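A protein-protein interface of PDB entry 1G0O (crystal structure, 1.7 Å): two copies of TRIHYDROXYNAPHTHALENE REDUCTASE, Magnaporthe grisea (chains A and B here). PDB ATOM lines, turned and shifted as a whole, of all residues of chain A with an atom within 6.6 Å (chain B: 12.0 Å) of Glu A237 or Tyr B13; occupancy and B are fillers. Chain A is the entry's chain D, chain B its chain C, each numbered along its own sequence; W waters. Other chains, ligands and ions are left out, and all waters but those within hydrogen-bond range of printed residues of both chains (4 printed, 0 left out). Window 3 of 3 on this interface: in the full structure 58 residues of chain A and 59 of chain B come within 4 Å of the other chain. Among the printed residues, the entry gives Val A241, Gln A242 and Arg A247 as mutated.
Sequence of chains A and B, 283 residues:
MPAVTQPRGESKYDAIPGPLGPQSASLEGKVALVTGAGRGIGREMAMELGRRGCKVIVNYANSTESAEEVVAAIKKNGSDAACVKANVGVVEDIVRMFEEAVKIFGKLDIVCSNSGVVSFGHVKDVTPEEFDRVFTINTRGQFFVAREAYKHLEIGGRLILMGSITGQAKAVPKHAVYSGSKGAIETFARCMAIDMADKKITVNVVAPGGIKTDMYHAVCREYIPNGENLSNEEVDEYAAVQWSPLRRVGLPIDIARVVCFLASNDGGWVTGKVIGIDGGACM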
ATOM      1  N   LYS A 212      -6.360  11.177  -7.892  1.00  0.00           N
ATOM      2  CA  LYS A 212      -6.178  10.316  -9.079  1.00  0.00           C
ATOM      3  C   LYS A 212      -5.931   8.836  -8.793  1.00  0.00           C
ATOM      4  O   LYS A 212      -4.829   8.432  -8.403  1.00  0.00           O
ATOM      5  CB  LYS A 212      -5.062  10.828  -9.997  1.00  0.00           C
ATOM      6  CG  LYS A 212      -5.420  12.047 -10.788  1.00  0.00           C
ATOM      7  CD  LYS A 212      -4.475  12.242 -11.975  1.00  0.00           C
ATOM      8  CE  LYS A 212      -4.695  11.174 -13.021  1.00  0.00           C
ATOM      9  NZ  LYS A 212      -3.909  11.461 -14.246  1.00  0.00           N
ATOM     10  N   TYR A 216     -11.300   7.577  -9.301  1.00  0.00           N
ATOM     11  CA  TYR A 216     -11.378   8.929  -9.857  1.00  0.00           C
ATOM     12  C   TYR A 216     -11.548   8.830 -11.373  1.00  0.00           C
ATOM     13  O   TYR A 216     -12.342   9.538 -11.983  1.00  0.00           O
ATOM     14  CB  TYR A 216     -10.095   9.684  -9.498  1.00  0.00           C
ATOM     15  CG  TYR A 216      -9.801  10.978 -10.253  1.00  0.00           C
ATOM     16  CD1 TYR A 216      -9.906  12.220  -9.613  1.00  0.00           C
ATOM     17  CD2 TYR A 216      -9.281  10.951 -11.562  1.00  0.00           C
ATOM     18  CE1 TYR A 216      -9.485  13.406 -10.247  1.00  0.00           C
ATOM     19  CE2 TYR A 216      -8.863  12.119 -12.208  1.00  0.00           C
ATOM     20  CZ  TYR A 216      -8.960  13.344 -11.544  1.00  0.00           C
ATOM     21  OH  TYR A 216      -8.512  14.491 -12.166  1.00  0.00           O
ATOM     22  N   ASN A 232      -9.390  12.871 -20.799  1.00  0.00           N
ATOM     23  CA  ASN A 232      -8.726  12.609 -19.532  1.00  0.00           C
ATOM     24  C   ASN A 232      -7.910  13.838 -19.093  1.00  0.00           C
ATOM     25  O   ASN A 232      -7.895  14.190 -17.908  1.00  0.00           O
ATOM     26  CB  ASN A 232      -7.816  11.382 -19.646  1.00  0.00           C
ATOM     27  CG  ASN A 232      -8.593  10.077 -19.750  1.00  0.00           C
ATOM     28  OD1 ASN A 232      -9.806  10.043 -19.557  1.00  0.00           O
ATOM     29  ND2 ASN A 232      -7.885   8.991 -20.032  1.00  0.00           N
ATOM     30  N   GLU A 233      -7.283  14.511 -20.066  1.00  0.00           N
ATOM     31  CA  GLU A 233      -6.464  15.695 -19.812  1.00  0.00           C
ATOM     32  C   GLU A 233      -7.321  16.856 -19.378  1.00  0.00           C
ATOM     33  O   GLU A 233      -6.944  17.594 -18.480  1.00  0.00           O
ATOM     34  CB  GLU A 233      -5.604  16.102 -21.029  1.00  0.00           C
ATOM     35  CG  GLU A 233      -5.863  15.368 -22.364  1.00  0.00           C
ATOM     36  CD  GLU A 233      -5.663  13.841 -22.314  1.00  0.00           C
ATOM     37  OE1 GLU A 233      -4.972  13.352 -21.410  1.00  0.00           O
ATOM     38  OE2 GLU A 233      -6.206  13.117 -23.170  1.00  0.00           O
ATOM     39  N   GLU A 234      -8.471  17.021 -20.019  1.00  0.00           N
ATOM     40  CA  GLU A 234      -9.391  18.094 -19.661  1.00  0.00           C
ATOM     41  C   GLU A 234      -9.983  17.863 -18.270  1.00  0.00           C
ATOM     42  O   GLU A 234     -10.258  18.812 -17.550  1.00  0.00           O
ATOM     43  CB  GLU A 234     -10.500  18.215 -20.701  1.00  0.00           C
ATOM     44  CG  GLU A 234      -9.981  18.703 -22.046  1.00  0.00           C
ATOM     45  CD  GLU A 234     -11.041  18.701 -23.129  1.00  0.00           C
ATOM     46  OE1 GLU A 234     -11.827  17.737 -23.201  1.00  0.00           O
ATOM     47  OE2 GLU A 234     -11.090  19.671 -23.911  1.00  0.00           O
ATOM     48  N   VAL A 235     -10.168  16.598 -17.899  1.00  0.00           N
ATOM     49  CA  VAL A 235     -10.709  16.251 -16.573  1.00  0.00           C
ATOM     50  C   VAL A 235      -9.724  16.687 -15.473  1.00  0.00           C
ATOM     51  O   VAL A 235     -10.110  17.346 -14.508  1.00  0.00           O
ATOM     52  CB  VAL A 235     -11.030  14.737 -16.475  1.00  0.00           C
ATOM     53  CG1 VAL A 235     -11.324  14.338 -15.025  1.00  0.00           C
ATOM     54  CG2 VAL A 235     -12.237  14.409 -17.366  1.00  0.00           C
ATOM     55  N   ASP A 236      -8.446  16.369 -15.672  1.00  0.00           N
ATOM     56  CA  ASP A 236      -7.387  16.744 -14.739  1.00  0.00           C
ATOM     57  C   ASP A 236      -7.243  18.261 -14.642  1.00  0.00           C
ATOM     58  O   ASP A 236      -7.049  18.799 -13.555  1.00  0.00           O
ATOM     59  CB  ASP A 236      -6.051  16.142 -15.178  1.00  0.00           C
ATOM     60  CG  ASP A 236      -5.937  14.659 -14.866  1.00  0.00           C
ATOM     61  OD1 ASP A 236      -6.912  14.049 -14.371  1.00  0.00           O
ATOM     62  OD2 ASP A 236      -4.852  14.103 -15.111  1.00  0.00           O
ATOM     63  N   GLU A 237      -7.321  18.946 -15.780  1.00  0.00           N
ATOM     64  CA  GLU A 237      -7.221  20.400 -15.786  1.00  0.00           C
ATOM     65  C   GLU A 237      -8.391  20.991 -14.982  1.00  0.00           C
ATOM     66  O   GLU A 237      -8.201  21.924 -14.190  1.00  0.00           O
ATOM     67  CB  GLU A 237      -7.221  20.935 -17.222  1.00  0.00           C
ATOM     68  CG  GLU A 237      -6.986  22.443 -17.337  1.00  0.00           C
ATOM     69  CD  GLU A 237      -5.633  22.908 -16.775  1.00  0.00           C
ATOM     70  OE1 GLU A 237      -5.510  24.103 -16.450  1.00  0.00           O
ATOM     71  OE2 GLU A 237      -4.688  22.101 -16.673  1.00  0.00           O
ATOM     72  N   TYR A 238      -9.586  20.418 -15.161  1.00  0.00           N
ATOM     73  CA  TYR A 238     -10.780  20.872 -14.437  1.00  0.00           C
ATOM     74  C   TYR A 238     -10.606  20.678 -12.926  1.00  0.00           C
ATOM     75  O   TYR A 238     -10.872  21.590 -12.136  1.00  0.00           O
ATOM     76  CB  TYR A 238     -12.036  20.112 -14.894  1.00  0.00           C
ATOM     77  CG  TYR A 238     -13.300  20.613 -14.201  1.00  0.00           C
ATOM     78  CD1 TYR A 238     -13.682  20.119 -12.950  1.00  0.00           C
ATOM     79  CD2 TYR A 238     -14.087  21.615 -14.784  1.00  0.00           C
ATOM     80  CE1 TYR A 238     -14.817  20.612 -12.293  1.00  0.00           C
ATOM     81  CE2 TYR A 238     -15.220  22.111 -14.141  1.00  0.00           C
ATOM     82  CZ  TYR A 238     -15.579  21.606 -12.897  1.00  0.00           C
ATOM     83  OH  TYR A 238     -16.694  22.094 -12.266  1.00  0.00           O
ATOM     84  N   ALA A 239     -10.198  19.472 -12.539  1.00  0.00           N
ATOM     85  CA  ALA A 239      -9.973  19.135 -11.135  1.00  0.00           C
ATOM     86  C   ALA A 239      -8.930  20.082 -10.505  1.00  0.00           C
ATOM     87  O   ALA A 239      -9.126  20.608  -9.403  1.00  0.00           O
ATOM     88  CB  ALA A 239      -9.522  17.662 -11.009  1.00  0.00           C
ATOM     89  N   ALA A 240      -7.846  20.327 -11.241  1.00  0.00           N
ATOM     90  CA  ALA A 240      -6.764  21.201 -10.788  1.00  0.00           C
ATOM     91  C   ALA A 240      -7.189  22.652 -10.530  1.00  0.00           C
ATOM     92  O   ALA A 240      -6.840  23.241  -9.509  1.00  0.00           O
ATOM     93  CB  ALA A 240      -5.624  21.168 -11.801  1.00  0.00           C
ATOM     94  N   VAL A 241      -7.952  23.214 -11.455  1.00  0.00           N
ATOM     95  CA  VAL A 241      -8.407  24.599 -11.358  1.00  0.00           C
ATOM     96  C   VAL A 241      -9.677  24.805 -10.520  1.00  0.00           C
ATOM     97  O   VAL A 241      -9.737  25.696  -9.678  1.00  0.00           O
ATOM     98  CB  VAL A 241      -8.632  25.198 -12.788  1.00  0.00           C
ATOM     99  CG1 VAL A 241      -9.090  26.645 -12.702  1.00  0.00           C
ATOM    100  CG2 VAL A 241      -7.350  25.078 -13.608  1.00  0.00           C
ATOM    101  N   GLN A 242     -10.697  23.991 -10.761  1.00  0.00           N
ATOM    102  CA  GLN A 242     -11.943  24.128 -10.032  1.00  0.00           C
ATOM    103  C   GLN A 242     -11.887  23.744  -8.563  1.00  0.00           C
ATOM    104  O   GLN A 242     -12.474  24.431  -7.738  1.00  0.00           O
ATOM    105  CB  GLN A 242     -13.047  23.307 -10.706  1.00  0.00           C
ATOM    106  CG  GLN A 242     -14.410  23.469 -10.060  1.00  0.00           C
ATOM    107  CD  GLN A 242     -14.917  24.908 -10.102  1.00  0.00           C
ATOM    108  OE1 GLN A 242     -15.547  25.393  -9.149  1.00  0.00           O
ATOM    109  NE2 GLN A 242     -14.662  25.592 -11.208  1.00  0.00           N
ATOM    110  N   ARG A 247      -4.024  24.881  -7.684  1.00  0.00           N
ATOM    111  CA  ARG A 247      -3.983  24.512  -9.109  1.00  0.00           C
ATOM    112  C   ARG A 247      -3.322  23.217  -9.526  1.00  0.00           C
ATOM    113  O   ARG A 247      -2.511  23.190 -10.456  1.00  0.00           O
ATOM    114  CB  ARG A 247      -3.417  25.671  -9.937  1.00  0.00           C
ATOM    115  CG  ARG A 247      -4.238  26.925  -9.793  1.00  0.00           C
ATOM    116  CD  ARG A 247      -3.692  28.055 -10.630  1.00  0.00           C
ATOM    117  NE  ARG A 247      -4.607  28.413 -11.721  1.00  0.00           N
ATOM    118  CZ  ARG A 247      -4.452  28.033 -12.989  1.00  0.00           C
ATOM    119  NH1 ARG A 247      -3.419  27.275 -13.342  1.00  0.00           N
ATOM    120  NH2 ARG A 247      -5.331  28.416 -13.912  1.00  0.00           N
ATOM    121  N   ARG A 248      -3.639  22.146  -8.808  1.00  0.00           N
ATOM    122  CA  ARG A 248      -3.141  20.822  -9.142  1.00  0.00           C
ATOM    123  C   ARG A 248      -4.142  19.759  -8.685  1.00  0.00           C
ATOM    124  O   ARG A 248      -5.102  20.059  -7.954  1.00  0.00           O
ATOM    125  CB  ARG A 248      -1.733  20.544  -8.578  1.00  0.00           C
ATOM    126  CG  ARG A 248      -1.648  20.239  -7.099  1.00  0.00           C
ATOM    127  CD  ARG A 248      -0.264  19.717  -6.788  1.00  0.00           C
ATOM    128  NE  ARG A 248      -0.011  19.548  -5.360  1.00  0.00           N
ATOM    129  CZ  ARG A 248      -0.365  18.483  -4.652  1.00  0.00           C
ATOM    130  NH1 ARG A 248      -1.012  17.481  -5.237  1.00  0.00           N
ATOM    131  NH2 ARG A 248       0.003  18.386  -3.378  1.00  0.00           N
ATOM    132  N   VAL A 249      -3.940  18.536  -9.171  1.00  0.00           N
ATOM    133  CA  VAL A 249      -4.806  17.411  -8.842  1.00  0.00           C
ATOM    134  C   VAL A 249      -4.284  16.676  -7.602  1.00  0.00           C
ATOM    135  O   VAL A 249      -3.079  16.590  -7.386  1.00  0.00           O
ATOM    136  CB  VAL A 249      -4.907  16.430 -10.058  1.00  0.00           C
ATOM    137  CG1 VAL A 249      -5.871  15.291  -9.756  1.00  0.00           C
ATOM    138  CG2 VAL A 249      -5.373  17.174 -11.294  1.00  0.00           C
ATOM    139  N   GLY A 250      -5.200  16.205  -6.762  1.00  0.00           N
ATOM    140  CA  GLY A 250      -4.811  15.465  -5.570  1.00  0.00           C
ATOM    141  C   GLY A 250      -4.280  14.092  -5.947  1.00  0.00           C
ATOM    142  O   GLY A 250      -4.786  13.453  -6.871  1.00  0.00           O
ATOM    143  N   LEU A 251      -3.268  13.633  -5.222  1.00  0.00           N
ATOM    144  CA  LEU A 251      -2.638  12.341  -5.493  1.00  0.00           C
ATOM    145  C   LEU A 251      -2.618  11.439  -4.260  1.00  0.00           C
ATOM    146  O   LEU A 251      -2.670  11.926  -3.125  1.00  0.00           O
ATOM    147  CB  LEU A 251      -1.209  12.567  -6.008  1.00  0.00           C
ATOM    148  CG  LEU A 251      -1.100  13.419  -7.280  1.00  0.00           C
ATOM    149  CD1 LEU A 251       0.357  13.811  -7.554  1.00  0.00           C
ATOM    150  CD2 LEU A 251      -1.697  12.664  -8.462  1.00  0.00           C
ATOM    151  N   ARG B   8      -6.265   5.119 -17.690  1.00  0.00           N
ATOM    152  CA  ARG B   8      -5.490   6.038 -16.858  1.00  0.00           C
ATOM    153  C   ARG B   8      -4.029   5.996 -17.248  1.00  0.00           C
ATOM    154  O   ARG B   8      -3.457   4.911 -17.431  1.00  0.00           O
ATOM    155  CB  ARG B   8      -5.568   5.645 -15.377  1.00  0.00           C
ATOM    156  CG  ARG B   8      -6.263   6.663 -14.521  1.00  0.00           C
ATOM    157  CD  ARG B   8      -5.673   6.746 -13.142  1.00  0.00           C
ATOM    158  NE  ARG B   8      -5.458   5.435 -12.536  1.00  0.00           N
ATOM    159  CZ  ARG B   8      -4.534   5.215 -11.601  1.00  0.00           C
ATOM    160  NH1 ARG B   8      -3.762   6.222 -11.201  1.00  0.00           N
ATOM    161  NH2 ARG B   8      -4.414   4.025 -11.023  1.00  0.00           N
ATOM    162  N   GLY B   9      -3.437   7.180 -17.371  1.00  0.00           N
ATOM    163  CA  GLY B   9      -2.028   7.278 -17.716  1.00  0.00           C
ATOM    164  C   GLY B   9      -1.376   8.453 -16.995  1.00  0.00           C
ATOM    165  O   GLY B   9      -2.070   9.341 -16.444  1.00  0.00           O
ATOM    166  N   GLU B  10      -0.046   8.478 -16.966  1.00  0.00           N
ATOM    167  CA  GLU B  10       0.614   9.585 -16.290  1.00  0.00           C
ATOM    168  C   GLU B  10       0.559  10.858 -17.125  1.00  0.00           C
ATOM    169  O   GLU B  10       0.433  10.807 -18.363  1.00  0.00           O
ATOM    170  CB  GLU B  10       2.021   9.198 -15.864  1.00  0.00           C
ATOM    171  CG  GLU B  10       1.990   8.096 -14.795  1.00  0.00           C
ATOM    172  CD  GLU B  10       2.910   8.383 -13.611  1.00  0.00           C
ATOM    173  OE1 GLU B  10       3.880   9.183 -13.776  1.00  0.00           O
ATOM    174  OE2 GLU B  10       2.667   7.811 -12.505  1.00  0.00           O
ATOM    175  N   SER B  11       0.487  11.991 -16.433  1.00  0.00           N
ATOM    176  CA  SER B  11       0.411  13.303 -17.077  1.00  0.00           C
ATOM    177  C   SER B  11       1.192  14.284 -16.214  1.00  0.00           C
ATOM    178  O   SER B  11       1.842  13.870 -15.242  1.00  0.00           O
ATOM    179  CB  SER B  11      -1.050  13.756 -17.193  1.00  0.00           C
ATOM    180  OG  SER B  11      -1.635  14.001 -15.922  1.00  0.00           O
ATOM    181  N   LYS B  12       1.129  15.574 -16.550  1.00  0.00           N
ATOM    182  CA  LYS B  12       1.851  16.570 -15.763  1.00  0.00           C
ATOM    183  C   LYS B  12       1.326  16.608 -14.327  1.00  0.00           C
ATOM    184  O   LYS B  12       2.086  16.851 -13.384  1.00  0.00           O
ATOM    185  CB  LYS B  12       1.784  17.966 -16.400  1.00  0.00           C
ATOM    186  CG  LYS B  12       0.425  18.642 -16.389  1.00  0.00           C
ATOM    187  CD  LYS B  12       0.568  20.103 -16.811  1.00  0.00           C
ATOM    188  CE  LYS B  12      -0.781  20.794 -16.989  1.00  0.00           C
ATOM    189  NZ  LYS B  12      -0.659  22.242 -17.363  1.00  0.00           N
ATOM    190  N   TYR B  13       0.043  16.292 -14.170  1.00  0.00           N
ATOM    191  CA  TYR B  13      -0.596  16.288 -12.862  1.00  0.00           C
ATOM    192  C   TYR B  13      -0.297  15.052 -12.015  1.00  0.00           C
ATOM    193  O   TYR B  13      -0.795  14.906 -10.896  1.00  0.00           O
ATOM    194  CB  TYR B  13      -2.090  16.532 -13.023  1.00  0.00           C
ATOM    195  CG  TYR B  13      -2.389  17.961 -13.434  1.00  0.00           C
ATOM    196  CD1 TYR B  13      -3.116  18.243 -14.595  1.00  0.00           C
ATOM    197  CD2 TYR B  13      -1.972  19.033 -12.640  1.00  0.00           C
ATOM    198  CE1 TYR B  13      -3.427  19.547 -14.953  1.00  0.00           C
ATOM    199  CE2 TYR B  13      -2.281  20.347 -12.989  1.00  0.00           C
ATOM    200  CZ  TYR B  13      -3.007  20.596 -14.144  1.00  0.00           C
ATOM    201  OH  TYR B  13      -3.305  21.892 -14.477  1.00  0.00           O
ATOM    202  N   ASP B  14       0.570  14.191 -12.531  1.00  0.00           N
ATOM    203  CA  ASP B  14       0.967  12.994 -11.808  1.00  0.00           C
ATOM    204  C   ASP B  14       2.302  13.175 -11.089  1.00  0.00           C
ATOM    205  O   ASP B  14       2.710  12.319 -10.302  1.00  0.00           O
ATOM    206  CB  ASP B  14       0.977  11.782 -12.742  1.00  0.00           C
ATOM    207  CG  ASP B  14      -0.430  11.262 -13.021  1.00  0.00           C
ATOM    208  OD1 ASP B  14      -1.018  11.656 -14.050  1.00  0.00           O
ATOM    209  OD2 ASP B  14      -0.957  10.476 -12.189  1.00  0.00           O
ATOM    210  N   ALA B  15       2.925  14.340 -11.293  1.00  0.00           N
ATOM    211  CA  ALA B  15       4.199  14.660 -10.666  1.00  0.00           C
ATOM    212  C   ALA B  15       4.066  14.652  -9.146  1.00  0.00           C
ATOM    213  O   ALA B  15       3.158  15.262  -8.598  1.00  0.00           O
ATOM    214  CB  ALA B  15       4.683  16.008 -11.136  1.00  0.00           C
ATOM    215  N   ILE B  16       4.951  13.916  -8.480  1.00  0.00           N
ATOM    216  CA  ILE B  16       4.954  13.812  -7.018  1.00  0.00           C
ATOM    217  C   ILE B  16       5.537  15.092  -6.417  1.00  0.00           C
ATOM    218  O   ILE B  16       6.642  15.507  -6.770  1.00  0.00           O
ATOM    219  CB  ILE B  16       5.832  12.611  -6.524  1.00  0.00           C
ATOM    220  CG1 ILE B  16       5.347  11.287  -7.130  1.00  0.00           C
ATOM    221  CG2 ILE B  16       5.843  12.535  -5.004  1.00  0.00           C
ATOM    222  CD1 ILE B  16       3.921  10.907  -6.781  1.00  0.00           C
ATOM    223  N   PRO B  17       4.773  15.764  -5.540  1.00  0.00           N
ATOM    224  CA  PRO B  17       5.228  17.002  -4.889  1.00  0.00           C
ATOM    225  C   PRO B  17       6.144  16.621  -3.713  1.00  0.00           C
ATOM    226  O   PRO B  17       5.695  16.014  -2.736  1.00  0.00           O
ATOM    227  CB  PRO B  17       3.922  17.613  -4.358  1.00  0.00           C
ATOM    228  CG  PRO B  17       2.817  16.851  -5.085  1.00  0.00           C
ATOM    229  CD  PRO B  17       3.371  15.478  -5.200  1.00  0.00           C
ATOM    230  N   GLY B  18       7.428  16.946  -3.804  1.00  0.00           N
ATOM    231  CA  GLY B  18       8.314  16.602  -2.707  1.00  0.00           C
ATOM    232  C   GLY B  18       8.756  15.152  -2.677  1.00  0.00           C
ATOM    233  O   GLY B  18       8.267  14.325  -3.449  1.00  0.00           O
ATOM    234  N   LYS B 200       1.484  29.451  -3.582  1.00  0.00           N
ATOM    235  CA  LYS B 200       1.561  28.051  -3.109  1.00  0.00           C
ATOM    236  C   LYS B 200       1.737  27.919  -1.589  1.00  0.00           C
ATOM    237  O   LYS B 200       2.327  26.956  -1.096  1.00  0.00           O
ATOM    238  CB  LYS B 200       2.679  27.262  -3.806  1.00  0.00           C
ATOM    239  CG  LYS B 200       2.638  27.281  -5.312  1.00  0.00           C
ATOM    240  CD  LYS B 200       1.351  26.725  -5.877  1.00  0.00           C
ATOM    241  CE  LYS B 200       1.367  26.873  -7.394  1.00  0.00           C
ATOM    242  NZ  LYS B 200       0.178  26.284  -8.044  1.00  0.00           N
ATOM    243  N   TRP B 269      -1.124  19.045   1.076  1.00  0.00           N
ATOM    244  CA  TRP B 269      -2.488  19.050   0.558  1.00  0.00           C
ATOM    245  C   TRP B 269      -3.512  19.452   1.634  1.00  0.00           C
ATOM    246  O   TRP B 269      -4.724  19.369   1.418  1.00  0.00           O
ATOM    247  CB  TRP B 269      -2.816  17.688  -0.068  1.00  0.00           C
ATOM    248  CG  TRP B 269      -3.831  17.729  -1.176  1.00  0.00           C
ATOM    249  CD1 TRP B 269      -4.903  16.901  -1.323  1.00  0.00           C
ATOM    250  CD2 TRP B 269      -3.854  18.625  -2.302  1.00  0.00           C
ATOM    251  NE1 TRP B 269      -5.590  17.217  -2.468  1.00  0.00           N
ATOM    252  CE2 TRP B 269      -4.973  18.269  -3.093  1.00  0.00           C
ATOM    253  CE3 TRP B 269      -3.042  19.689  -2.727  1.00  0.00           C
ATOM    254  CZ2 TRP B 269      -5.302  18.938  -4.283  1.00  0.00           C
ATOM    255  CZ3 TRP B 269      -3.371  20.360  -3.921  1.00  0.00           C
ATOM    256  CH2 TRP B 269      -4.495  19.974  -4.680  1.00  0.00           C
HETATM  257  O   HOH W   1      -3.795  14.696 -17.762  1.00  0.00           O
HETATM  258  O   HOH W   2      -3.368  24.226 -12.796  1.00  0.00           O
HETATM  259  O   HOH W   3      -1.155  16.991  -9.223  1.00  0.00           O
HETATM  260  O   HOH W   4      -2.478   7.543  -8.911  1.00  0.00           O
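The side-chain hydroxyl (OG) of Ser B11 sits close to the backbone NH (N) of Tyr B13.
OD1 of Asp B14 lies within hydrogen-bond range of N of Ser B11, at 2.8 Å.
NZ of Lys A212 lies within salt-bridge range of OD2 of Asp A236 (2.9 Å).
O of Gly A250 is in hydrogen-bond range of N of Lys A212, 2.9 Å away.
The side-chain hydroxyl of Tyr A216 lies within hydrogen-bond range of the side-chain carboxylate of Asp A236 (2.8 Å).
The backbone carbonyl oxygen (O) of Ala A240 is in hydrogen-bond range of the backbone NH (N) of Arg A248.
Of the 13 printed residues of chain B, 8 touch a printed residue of chain A.
Hydrophobic or aromatic side chains of chain B within 4 Å of the printed part of chain A: Tyr B13, Pro B17 and Trp B269.
Of the 18 printed residues of chain A, 9 touch a printed residue of chain B.
Hydrophobic or aromatic side chains of chain A that line the printed part of chain B: Ala A240, Val A249 and Leu A251.
Among the printed residues, 17 pairs touch across the chains.
Among the printed residues, Asp or Glu carboxylates within 4 Å of a Lys or Arg side-chain nitrogen of the other chain: Lys A212 with Asp B14 (2.9 Å).
No position is printed for both chains.
OD2 of Asp A236 lies within hydrogen-bond range of OG of Ser B11 (3.3 Å).
OE2 of Glu A237 is in hydrogen-bond range of OH of Tyr B13.
The side-chain carboxylate (OD1) of Asp B14 lies within salt-bridge range of the side-chain amino group (NZ) of Lys A212.
Among the printed residues, merely in contact across the chains: Leu A251 with Ala B15, Arg A248 with Trp B269, Leu A251 with Tyr B13, Ala A240 with Tyr B13, Lys A212 with Gly B9, Arg A248 with Pro B17, Gly A250 with Trp B269, Asp A236 with Tyr B13, Lys A212 with Arg B8, Val A249 with Tyr B13, Lys A212 with Ser B11, Arg A247 with Tyr B13, Leu A251 with Asp B14 and Arg A248 with Tyr B13.
Of chain B, only Ser B11 (3.3 Å) and Tyr B13 (3.7 Å) come within 4 Å of Asp A236.
Ala A240 touches just one residue of chain B: Tyr B13 (3.6 Å).
Of chain B, only Tyr B13 (3.8 Å) comes within 4 Å of Arg A247.
Of the printed residues of chain B, Arg A248 touches Tyr B13, Pro B17 and Trp B269.
Of the printed residues of chain B, Gly A250 touches Trp B269.
Of the printed residues of chain A, Gly B9 touches Lys A212.
Tyr B13 touches just these residues of chain A: Asp A236, Glu A237, Ala A240, Arg A247, Arg A248, Val A249 and Leu A251.
Water W4 bridges O of Lys A212 (2.6 Å) and NH1 of Arg B8 (2.9 Å).
Water W3 bridges O of Val A249 (2.7 Å) and O of Tyr B13 (2.7 Å).
Water W2 bridges the backbone carbonyl oxygen (O) of Arg A247 and the side-chain hydroxyl (OH) of Tyr B13.
Water W1 bridges OD2 of Asp A236 (2.9 Å) and OG of Ser B11 (2.9 Å).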
